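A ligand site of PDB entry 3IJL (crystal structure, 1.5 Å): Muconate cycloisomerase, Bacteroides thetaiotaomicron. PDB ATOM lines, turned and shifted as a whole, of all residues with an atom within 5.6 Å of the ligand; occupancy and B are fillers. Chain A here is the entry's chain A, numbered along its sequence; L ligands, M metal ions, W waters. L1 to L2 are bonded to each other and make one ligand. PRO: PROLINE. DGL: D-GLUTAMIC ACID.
The side-chain carboxylate (OD1) of Asp 305 lies within salt-bridge range of a nitrogen (N) of PRO L1, 2.7 Å away.
OE2 of DGL L2 sits at hydrogen-bond distance from N of Thr 283.
An oxygen (OE2) of DGL L2 lies within salt-bridge range of the guanidinium group (NH2) of Arg 23.
The side-chain amino group of Lys 253 lies within salt-bridge range of an oxygen (OXT) of DGL L2.
N of PRO L1 lies within salt-bridge range of OD2 of Asp 303, 3.1 Å away.
The backbone carbonyl oxygen of Cys 281 lies within hydrogen-bond range of a nitrogen (N) of DGL L2 (2.9 Å).
An oxygen (O) of PRO L1 sits at hydrogen-bond distance from the side-chain amino group (NZ) of Lys 153 (3.3 Å).
OH of Tyr 49 is in hydrogen-bond range of OE1 of DGL L2 (2.6 Å).
SG of Cys 281 lies within hydrogen-bond range of O of Asp 303 (3.2 Å).
OD2 of Asp 303 lies within salt-bridge range of NZ of Lys 153 (3.0 Å).
The backbone NH (N) of Phe 16 sits at hydrogen-bond distance from the backbone carbonyl oxygen (O) of Arg 23 (2.8 Å).
The side-chain hydroxyl (OG1) of Thr 26 lies within hydrogen-bond range of the guanidinium group (NE) of Arg 23, 3.0 Å away.
The side-chain amino group of Lys 253 is in salt-bridge range of the side-chain carboxylate of Asp 231, at 3.2 Å.
OG1 of Thr 283 sits at hydrogen-bond distance from OG1 of Thr 26, 2.7 Å away.
The guanidinium group of Arg 23 is in hydrogen-bond range of the side-chain hydroxyl of Thr 283 (3.1 Å).
The side-chain sulfur (SG) of Cys 281 lies within hydrogen-bond range of the backbone NH (N) of Gly 306, at 3.3 Å.
CZ of Phe 16 touches O of PRO L1 (3.8 Å).
CG2 of Val 18 touches OE1 of DGL L2 (3.7 Å).
CB of Pro 47 touches OE1 of DGL L2 (3.6 Å).
Met 282 touches the ligand.
Gly 306 touches the ligand.
CD2 of Leu 309 touches CG of PRO L1, at 3.6 Å.
Hydrophobic or aromatic side chains that line the ligand: Phe 16, Val 18, Pro 47, Tyr 49, Met 282 and Leu 309.
14 residues have an atom within 4 Å of the ligand: Phe 16, Val 18, Arg 23, Pro 47, Tyr 49, Lys 153, Lys 253, Cys 281, Met 282, Thr 283, Asp 303, Asp 305, Gly 306 and Leu 309.
The nearest printed residue that does not touch the ligand is Thr 129 (4.3 Å).
Water W7 lies within hydrogen-bond range of O of PRO L1 (2.7 Å), OG1 of Thr 129 (2.8 Å) and NZ of Lys 155 (3.0 Å).
Water W1 bridges the side-chain hydroxyl (OH) of Tyr 49 (2.7 Å) and an oxygen (O) of DGL L2 (2.7 Å).
Water W3 lies within hydrogen-bond range of O of DGL L2 (2.8 Å), OD1 of Asn 181 (2.9 Å) and OE2 of Glu 232 (3.0 Å).
Water W2 bridges an oxygen (OXT) of DGL L2 (2.9 Å) and the side-chain amino group (NZ) of Lys 253 (3.3 Å).
Water W6 lies within hydrogen-bond range of the side-chain carboxylate of Asp 303 (2.6 Å), an oxygen (OXT) of DGL L2 (2.9 Å) and the backbone NH of Cys 281 (2.9 Å).
Water W4 lies within hydrogen-bond range of OG1 of Thr 129 (2.6 Å), OD1 of Asp 303 (2.7 Å), OD2 of Asp 305 (2.7 Å) and N of PRO L1 (2.9 Å).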
ATOM      1  N   PHE A  16       9.059   7.614  18.142  1.00  0.00           N
ATOM      2  CA  PHE A  16       9.105   8.747  17.220  1.00  0.00           C
ATOM      3  C   PHE A  16       8.736   8.254  15.832  1.00  0.00           C
ATOM      4  O   PHE A  16       9.304   7.282  15.339  1.00  0.00           O
ATOM      5  CB  PHE A  16      10.507   9.355  17.212  1.00  0.00           C
ATOM      6  CG  PHE A  16      10.628  10.594  16.367  1.00  0.00           C
ATOM      7  CD1 PHE A  16       9.908  11.738  16.688  1.00  0.00           C
ATOM      8  CD2 PHE A  16      11.460  10.613  15.254  1.00  0.00           C
ATOM      9  CE1 PHE A  16      10.010  12.887  15.900  1.00  0.00           C
ATOM     10  CE2 PHE A  16      11.574  11.756  14.466  1.00  0.00           C
ATOM     11  CZ  PHE A  16      10.842  12.893  14.786  1.00  0.00           C
ATOM     12  N   VAL A  18       8.086   9.139  11.641  1.00  0.00           N
ATOM     13  CA  VAL A  18       8.274   9.976  10.471  1.00  0.00           C
ATOM     14  C   VAL A  18       7.557   9.242   9.343  1.00  0.00           C
ATOM     15  O   VAL A  18       7.961   8.152   8.938  1.00  0.00           O
ATOM     16  CB  VAL A  18       9.768  10.127  10.100  1.00  0.00           C
ATOM     17  CG1 VAL A  18       9.916  11.038   8.895  1.00  0.00           C
ATOM     18  CG2 VAL A  18      10.534  10.678  11.290  1.00  0.00           C
ATOM     19  N   ARG A  23      10.231   4.594  15.407  1.00  0.00           N
ATOM     20  CA  ARG A  23      11.429   4.073  16.043  1.00  0.00           C
ATOM     21  C   ARG A  23      11.578   4.595  17.467  1.00  0.00           C
ATOM     22  O   ARG A  23      10.949   5.584  17.840  1.00  0.00           O
ATOM     23  CB  ARG A  23      12.674   4.433  15.223  1.00  0.00           C
ATOM     24  CG  ARG A  23      13.087   5.906  15.243  1.00  0.00           C
ATOM     25  CD  ARG A  23      14.337   6.099  14.387  1.00  0.00           C
ATOM     26  NE  ARG A  23      15.024   7.369  14.594  1.00  0.00           N
ATOM     27  CZ  ARG A  23      14.726   8.512  13.984  1.00  0.00           C
ATOM     28  NH1 ARG A  23      13.740   8.566  13.105  1.00  0.00           N
ATOM     29  NH2 ARG A  23      15.438   9.602  14.236  1.00  0.00           N
ATOM     30  N   THR A  26      18.106   5.774  17.687  1.00  0.00           N
ATOM     31  CA  THR A  26      18.705   6.309  16.478  1.00  0.00           C
ATOM     32  C   THR A  26      20.199   6.027  16.399  1.00  0.00           C
ATOM     33  O   THR A  26      20.963   6.401  17.298  1.00  0.00           O
ATOM     34  CB  THR A  26      18.519   7.850  16.396  1.00  0.00           C
ATOM     35  OG1 THR A  26      17.132   8.184  16.509  1.00  0.00           O
ATOM     36  CG2 THR A  26      19.045   8.366  15.065  1.00  0.00           C
ATOM     37  N   PRO A  47      19.159   8.551  10.968  1.00  0.00           N
ATOM     38  CA  PRO A  47      17.806   7.981  11.014  1.00  0.00           C
ATOM     39  C   PRO A  47      17.859   6.891   9.936  1.00  0.00           C
ATOM     40  O   PRO A  47      18.221   7.176   8.795  1.00  0.00           O
ATOM     41  CB  PRO A  47      16.928   9.160  10.624  1.00  0.00           C
ATOM     42  CG  PRO A  47      17.669  10.327  11.253  1.00  0.00           C
ATOM     43  CD  PRO A  47      19.110  10.032  10.905  1.00  0.00           C
ATOM     44  N   TYR A  49      15.896   5.442   7.760  1.00  0.00           N
ATOM     45  CA  TYR A  49      15.327   5.685   6.439  1.00  0.00           C
ATOM     46  C   TYR A  49      16.113   6.672   5.589  1.00  0.00           C
ATOM     47  O   TYR A  49      15.772   6.886   4.417  1.00  0.00           O
ATOM     48  CB  TYR A  49      13.873   6.152   6.585  1.00  0.00           C
ATOM     49  CG  TYR A  49      13.742   7.485   7.286  1.00  0.00           C
ATOM     50  CD1 TYR A  49      13.842   8.679   6.566  1.00  0.00           C
ATOM     51  CD2 TYR A  49      13.545   7.555   8.663  1.00  0.00           C
ATOM     52  CE1 TYR A  49      13.751   9.901   7.213  1.00  0.00           C
ATOM     53  CE2 TYR A  49      13.458   8.784   9.317  1.00  0.00           C
ATOM     54  CZ  TYR A  49      13.561   9.944   8.582  1.00  0.00           C
ATOM     55  OH  TYR A  49      13.494  11.167   9.211  1.00  0.00           O
ATOM     56  N   THR A 129       7.343  19.396  18.127  1.00  0.00           N
ATOM     57  CA  THR A 129       6.294  18.640  17.465  1.00  0.00           C
ATOM     58  C   THR A 129       5.181  18.068  18.339  1.00  0.00           C
ATOM     59  O   THR A 129       5.419  17.578  19.438  1.00  0.00           O
ATOM     60  CB  THR A 129       6.889  17.485  16.651  1.00  0.00           C
ATOM     61  OG1 THR A 129       7.701  18.020  15.588  1.00  0.00           O
ATOM     62  CG2 THR A 129       5.790  16.613  16.049  1.00  0.00           C
ATOM     63  N   LYS A 153       5.066  22.550  15.721  1.00  0.00           N
ATOM     64  CA  LYS A 153       5.183  21.871  14.443  1.00  0.00           C
ATOM     65  C   LYS A 153       4.224  20.685  14.392  1.00  0.00           C
ATOM     66  O   LYS A 153       4.039  19.989  15.399  1.00  0.00           O
ATOM     67  CB  LYS A 153       6.609  21.373  14.237  1.00  0.00           C
ATOM     68  CG  LYS A 153       6.792  20.468  13.024  1.00  0.00           C
ATOM     69  CD  LYS A 153       8.255  20.070  12.895  1.00  0.00           C
ATOM     70  CE  LYS A 153       8.490  19.110  11.752  1.00  0.00           C
ATOM     71  NZ  LYS A 153       9.939  18.798  11.606  1.00  0.00           N
ATOM     72  N   LYS A 155       3.138  17.418  11.666  1.00  0.00           N
ATOM     73  CA  LYS A 155       3.435  16.704  10.432  1.00  0.00           C
ATOM     74  C   LYS A 155       2.130  16.278   9.788  1.00  0.00           C
ATOM     75  O   LYS A 155       1.404  15.428  10.312  1.00  0.00           O
ATOM     76  CB  LYS A 155       4.324  15.497  10.733  1.00  0.00           C
ATOM     77  CG  LYS A 155       5.751  15.898  11.115  1.00  0.00           C
ATOM     78  CD  LYS A 155       6.596  14.727  11.597  1.00  0.00           C
ATOM     79  CE  LYS A 155       6.115  14.216  12.941  1.00  0.00           C
ATOM     80  NZ  LYS A 155       7.094  13.274  13.557  1.00  0.00           N
ATOM     81  N   ASP A 179       4.650  20.449   8.175  1.00  0.00           N
ATOM     82  CA  ASP A 179       5.534  19.744   7.257  1.00  0.00           C
ATOM     83  C   ASP A 179       4.672  18.648   6.651  1.00  0.00           C
ATOM     84  O   ASP A 179       4.274  17.702   7.343  1.00  0.00           O
ATOM     85  CB  ASP A 179       6.726  19.122   8.001  1.00  0.00           C
ATOM     86  CG  ASP A 179       7.773  18.581   7.044  1.00  0.00           C
ATOM     87  OD1 ASP A 179       7.428  18.334   5.878  1.00  0.00           O
ATOM     88  OD2 ASP A 179       8.932  18.395   7.468  1.00  0.00           O
ATOM     89  N   ASN A 181       5.636  16.679   4.231  1.00  0.00           N
ATOM     90  CA  ASN A 181       6.492  15.575   3.810  1.00  0.00           C
ATOM     91  C   ASN A 181       6.084  14.944   2.481  1.00  0.00           C
ATOM     92  O   ASN A 181       5.912  13.727   2.384  1.00  0.00           O
ATOM     93  CB  ASN A 181       6.524  14.493   4.898  1.00  0.00           C
ATOM     94  CG  ASN A 181       7.313  14.914   6.113  1.00  0.00           C
ATOM     95  OD1 ASN A 181       8.540  15.069   6.042  1.00  0.00           O
ATOM     96  ND2 ASN A 181       6.636  15.111   7.232  1.00  0.00           N
ATOM     97  N   GLU A 206       5.943  23.364   4.663  1.00  0.00           N
ATOM     98  CA  GLU A 206       7.174  22.692   4.275  1.00  0.00           C
ATOM     99  C   GLU A 206       6.902  21.487   3.374  1.00  0.00           C
ATOM    100  O   GLU A 206       6.042  20.650   3.673  1.00  0.00           O
ATOM    101  CB  GLU A 206       7.932  22.258   5.542  1.00  0.00           C
ATOM    102  CG  GLU A 206       9.235  21.530   5.307  1.00  0.00           C
ATOM    103  CD  GLU A 206       9.940  21.173   6.608  1.00  0.00           C
ATOM    104  OE1 GLU A 206      10.936  20.416   6.543  1.00  0.00           O
ATOM    105  OE2 GLU A 206       9.505  21.639   7.684  1.00  0.00           O
ATOM    106  N   ASP A 231      12.553  20.766   1.515  1.00  0.00           N
ATOM    107  CA  ASP A 231      13.300  19.899   2.413  1.00  0.00           C
ATOM    108  C   ASP A 231      13.768  18.697   1.607  1.00  0.00           C
ATOM    109  O   ASP A 231      14.919  18.639   1.172  1.00  0.00           O
ATOM    110  CB  ASP A 231      12.441  19.457   3.587  1.00  0.00           C
ATOM    111  CG  ASP A 231      13.226  18.671   4.631  1.00  0.00           C
ATOM    112  OD1 ASP A 231      14.388  18.317   4.354  1.00  0.00           O
ATOM    113  OD2 ASP A 231      12.676  18.407   5.716  1.00  0.00           O
ATOM    114  N   GLU A 232      12.866  17.744   1.370  1.00  0.00           N
ATOM    115  CA  GLU A 232      13.223  16.562   0.600  1.00  0.00           C
ATOM    116  C   GLU A 232      13.678  16.936  -0.806  1.00  0.00           C
ATOM    117  O   GLU A 232      14.364  16.145  -1.471  1.00  0.00           O
ATOM    118  CB  GLU A 232      12.031  15.596   0.506  1.00  0.00           C
ATOM    119  CG  GLU A 232      11.742  14.803   1.778  1.00  0.00           C
ATOM    120  CD  GLU A 232      11.378  15.671   2.959  1.00  0.00           C
ATOM    121  OE1 GLU A 232      10.565  16.599   2.771  1.00  0.00           O
ATOM    122  OE2 GLU A 232      11.899  15.430   4.071  1.00  0.00           O
ATOM    123  N   ASN A 251      15.329  24.361   3.461  1.00  0.00           N
ATOM    124  CA  ASN A 251      15.567  23.838   4.800  1.00  0.00           C
ATOM    125  C   ASN A 251      16.956  23.201   4.763  1.00  0.00           C
ATOM    126  O   ASN A 251      17.255  22.397   3.876  1.00  0.00           O
ATOM    127  CB  ASN A 251      14.519  22.779   5.169  1.00  0.00           C
ATOM    128  CG  ASN A 251      14.615  22.356   6.626  1.00  0.00           C
ATOM    129  OD1 ASN A 251      15.503  22.783   7.355  1.00  0.00           O
ATOM    130  ND2 ASN A 251      13.681  21.509   7.063  1.00  0.00           N
ATOM    131  N   LYS A 253      19.920  20.969   6.817  1.00  0.00           N
ATOM    132  CA  LYS A 253      20.171  20.045   7.930  1.00  0.00           C
ATOM    133  C   LYS A 253      21.617  19.576   7.807  1.00  0.00           C
ATOM    134  O   LYS A 253      22.045  19.138   6.739  1.00  0.00           O
ATOM    135  CB  LYS A 253      19.220  18.858   7.890  1.00  0.00           C
ATOM    136  CG  LYS A 253      17.757  19.246   7.966  1.00  0.00           C
ATOM    137  CD  LYS A 253      16.854  18.016   7.923  1.00  0.00           C
ATOM    138  CE  LYS A 253      15.437  18.401   7.542  1.00  0.00           C
ATOM    139  NZ  LYS A 253      14.547  17.216   7.381  1.00  0.00           N
ATOM    140  N   GLY A 280      16.772  22.585  10.182  1.00  0.00           N
ATOM    141  CA  GLY A 280      16.155  21.466  10.866  1.00  0.00           C
ATOM    142  C   GLY A 280      17.204  20.573  11.480  1.00  0.00           C
ATOM    143  O   GLY A 280      18.390  20.914  11.498  1.00  0.00           O
ATOM    144  N   CYS A 281      16.788  19.416  11.959  1.00  0.00           N
ATOM    145  CA  CYS A 281      17.710  18.488  12.599  1.00  0.00           C
ATOM    146  C   CYS A 281      17.095  17.107  12.714  1.00  0.00           C
ATOM    147  O   CYS A 281      15.904  16.924  12.488  1.00  0.00           O
ATOM    148  CB  CYS A 281      18.046  18.965  14.008  1.00  0.00           C
ATOM    149  SG  CYS A 281      16.618  18.924  15.158  1.00  0.00           S
ATOM    150  N   MET A 282      17.939  16.137  13.066  1.00  0.00           N
ATOM    151  CA  MET A 282      17.479  14.773  13.299  1.00  0.00           C
ATOM    152  C   MET A 282      17.519  14.666  14.813  1.00  0.00           C
ATOM    153  O   MET A 282      17.892  15.615  15.499  1.00  0.00           O
ATOM    154  CB  MET A 282      18.459  13.750  12.727  1.00  0.00           C
ATOM    155  CG  MET A 282      18.960  14.023  11.331  1.00  0.00           C
ATOM    156  SD  MET A 282      17.609  14.120  10.158  1.00  0.00           S
ATOM    157  CE  MET A 282      18.483  14.716   8.718  1.00  0.00           C
ATOM    158  N   THR A 283      17.114  13.512  15.345  1.00  0.00           N
ATOM    159  CA  THR A 283      17.230  13.317  16.790  1.00  0.00           C
ATOM    160  C   THR A 283      18.761  13.289  16.914  1.00  0.00           C
ATOM    161  O   THR A 283      19.418  12.459  16.293  1.00  0.00           O
ATOM    162  CB  THR A 283      16.635  11.962  17.213  1.00  0.00           C
ATOM    163  OG1 THR A 283      17.215  10.919  16.419  1.00  0.00           O
ATOM    164  CG2 THR A 283      15.121  11.966  17.023  1.00  0.00           C
ATOM    165  N   ASP A 303      13.779  24.203  13.489  1.00  0.00           N
ATOM    166  CA  ASP A 303      13.275  23.011  14.174  1.00  0.00           C
ATOM    167  C   ASP A 303      14.584  22.472  14.740  1.00  0.00           C
ATOM    168  O   ASP A 303      15.253  21.649  14.119  1.00  0.00           O
ATOM    169  CB  ASP A 303      12.648  22.018  13.177  1.00  0.00           C
ATOM    170  CG  ASP A 303      11.881  20.908  13.873  1.00  0.00           C
ATOM    171  OD1 ASP A 303      11.072  21.216  14.773  1.00  0.00           O
ATOM    172  OD2 ASP A 303      12.066  19.726  13.518  1.00  0.00           O
ATOM    173  N   ASP A 305      15.161  21.046  18.016  1.00  0.00           N
ATOM    174  CA  ASP A 305      14.756  20.420  19.271  1.00  0.00           C
ATOM    175  C   ASP A 305      15.156  18.947  19.347  1.00  0.00           C
ATOM    176  O   ASP A 305      14.693  18.223  20.217  1.00  0.00           O
ATOM    177  CB  ASP A 305      13.239  20.521  19.395  1.00  0.00           C
ATOM    178  CG  ASP A 305      12.518  19.780  18.277  1.00  0.00           C
ATOM    179  OD1 ASP A 305      13.146  19.594  17.212  1.00  0.00           O
ATOM    180  OD2 ASP A 305      11.348  19.396  18.453  1.00  0.00           O
ATOM    181  N   GLY A 306      16.016  18.519  18.426  1.00  0.00           N
ATOM    182  CA  GLY A 306      16.413  17.119  18.380  1.00  0.00           C
ATOM    183  C   GLY A 306      16.922  16.475  19.666  1.00  0.00           C
ATOM    184  O   GLY A 306      16.641  15.298  19.918  1.00  0.00           O
ATOM    185  N   LEU A 309      14.395  15.117  22.456  1.00  0.00           N
ATOM    186  CA  LEU A 309      13.736  13.820  22.305  1.00  0.00           C
ATOM    187  C   LEU A 309      14.585  12.633  22.722  1.00  0.00           C
ATOM    188  O   LEU A 309      14.109  11.495  22.682  1.00  0.00           O
ATOM    189  CB  LEU A 309      13.238  13.624  20.870  1.00  0.00           C
ATOM    190  CG  LEU A 309      11.949  14.361  20.498  1.00  0.00           C
ATOM    191  CD1 LEU A 309      12.195  15.864  20.455  1.00  0.00           C
ATOM    192  CD2 LEU A 309      11.437  13.859  19.168  1.00  0.00           C
HETATM  193  N   PRO L   1      12.322  17.524  15.688  1.00  0.00           N
HETATM  194  CA  PRO L   1      13.281  17.102  14.663  1.00  0.00           C
HETATM  195  C   PRO L   1      12.440  16.479  13.520  1.00  0.00           C
HETATM  196  O   PRO L   1      11.206  16.437  13.588  1.00  0.00           O
HETATM  197  CB  PRO L   1      14.148  16.076  15.394  1.00  0.00           C
HETATM  198  CG  PRO L   1      13.167  15.429  16.385  1.00  0.00           C
HETATM  199  CD  PRO L   1      12.292  16.594  16.834  1.00  0.00           C
HETATM  200  N   DGL L   2      13.128  16.007  12.473  1.00  0.00           N
HETATM  201  CA  DGL L   2      12.457  15.279  11.357  1.00  0.00           C
HETATM  202  C   DGL L   2      12.808  15.865   9.989  1.00  0.00           C
HETATM  203  O   DGL L   2      12.356  15.289   8.966  1.00  0.00           O
HETATM  204  CB  DGL L   2      12.831  13.778  11.431  1.00  0.00           C
HETATM  205  CG  DGL L   2      14.328  13.436  11.492  1.00  0.00           C
HETATM  206  CD  DGL L   2      14.607  12.144  12.206  1.00  0.00           C
HETATM  207  OE1 DGL L   2      14.153  11.072  11.748  1.00  0.00           O
HETATM  208  OE2 DGL L   2      15.287  12.189  13.248  1.00  0.00           O
HETATM  209  OXT DGL L   2      13.508  16.900   9.925  1.00  0.00           O
HETATM  210 MG    MG M   1      10.825  18.440   6.545  1.00  0.00          MG
HETATM  211  O   HOH W   1      13.628  13.309   7.577  1.00  0.00           O
HETATM  212  O   HOH W   2      11.672  18.536   8.472  1.00  0.00           O
HETATM  213  O   HOH W   3      11.046  16.313   6.769  1.00  0.00           O
HETATM  214  O   HOH W   4       9.978  19.211  16.124  1.00  0.00           O
HETATM  215  O   HOH W   5       9.587  14.351   9.431  1.00  0.00           O
HETATM  216  O   HOH W   6      13.881  19.167  11.670  1.00  0.00           O
HETATM  217  O   HOH W   7       8.687  15.797  14.180  1.00  0.00           O
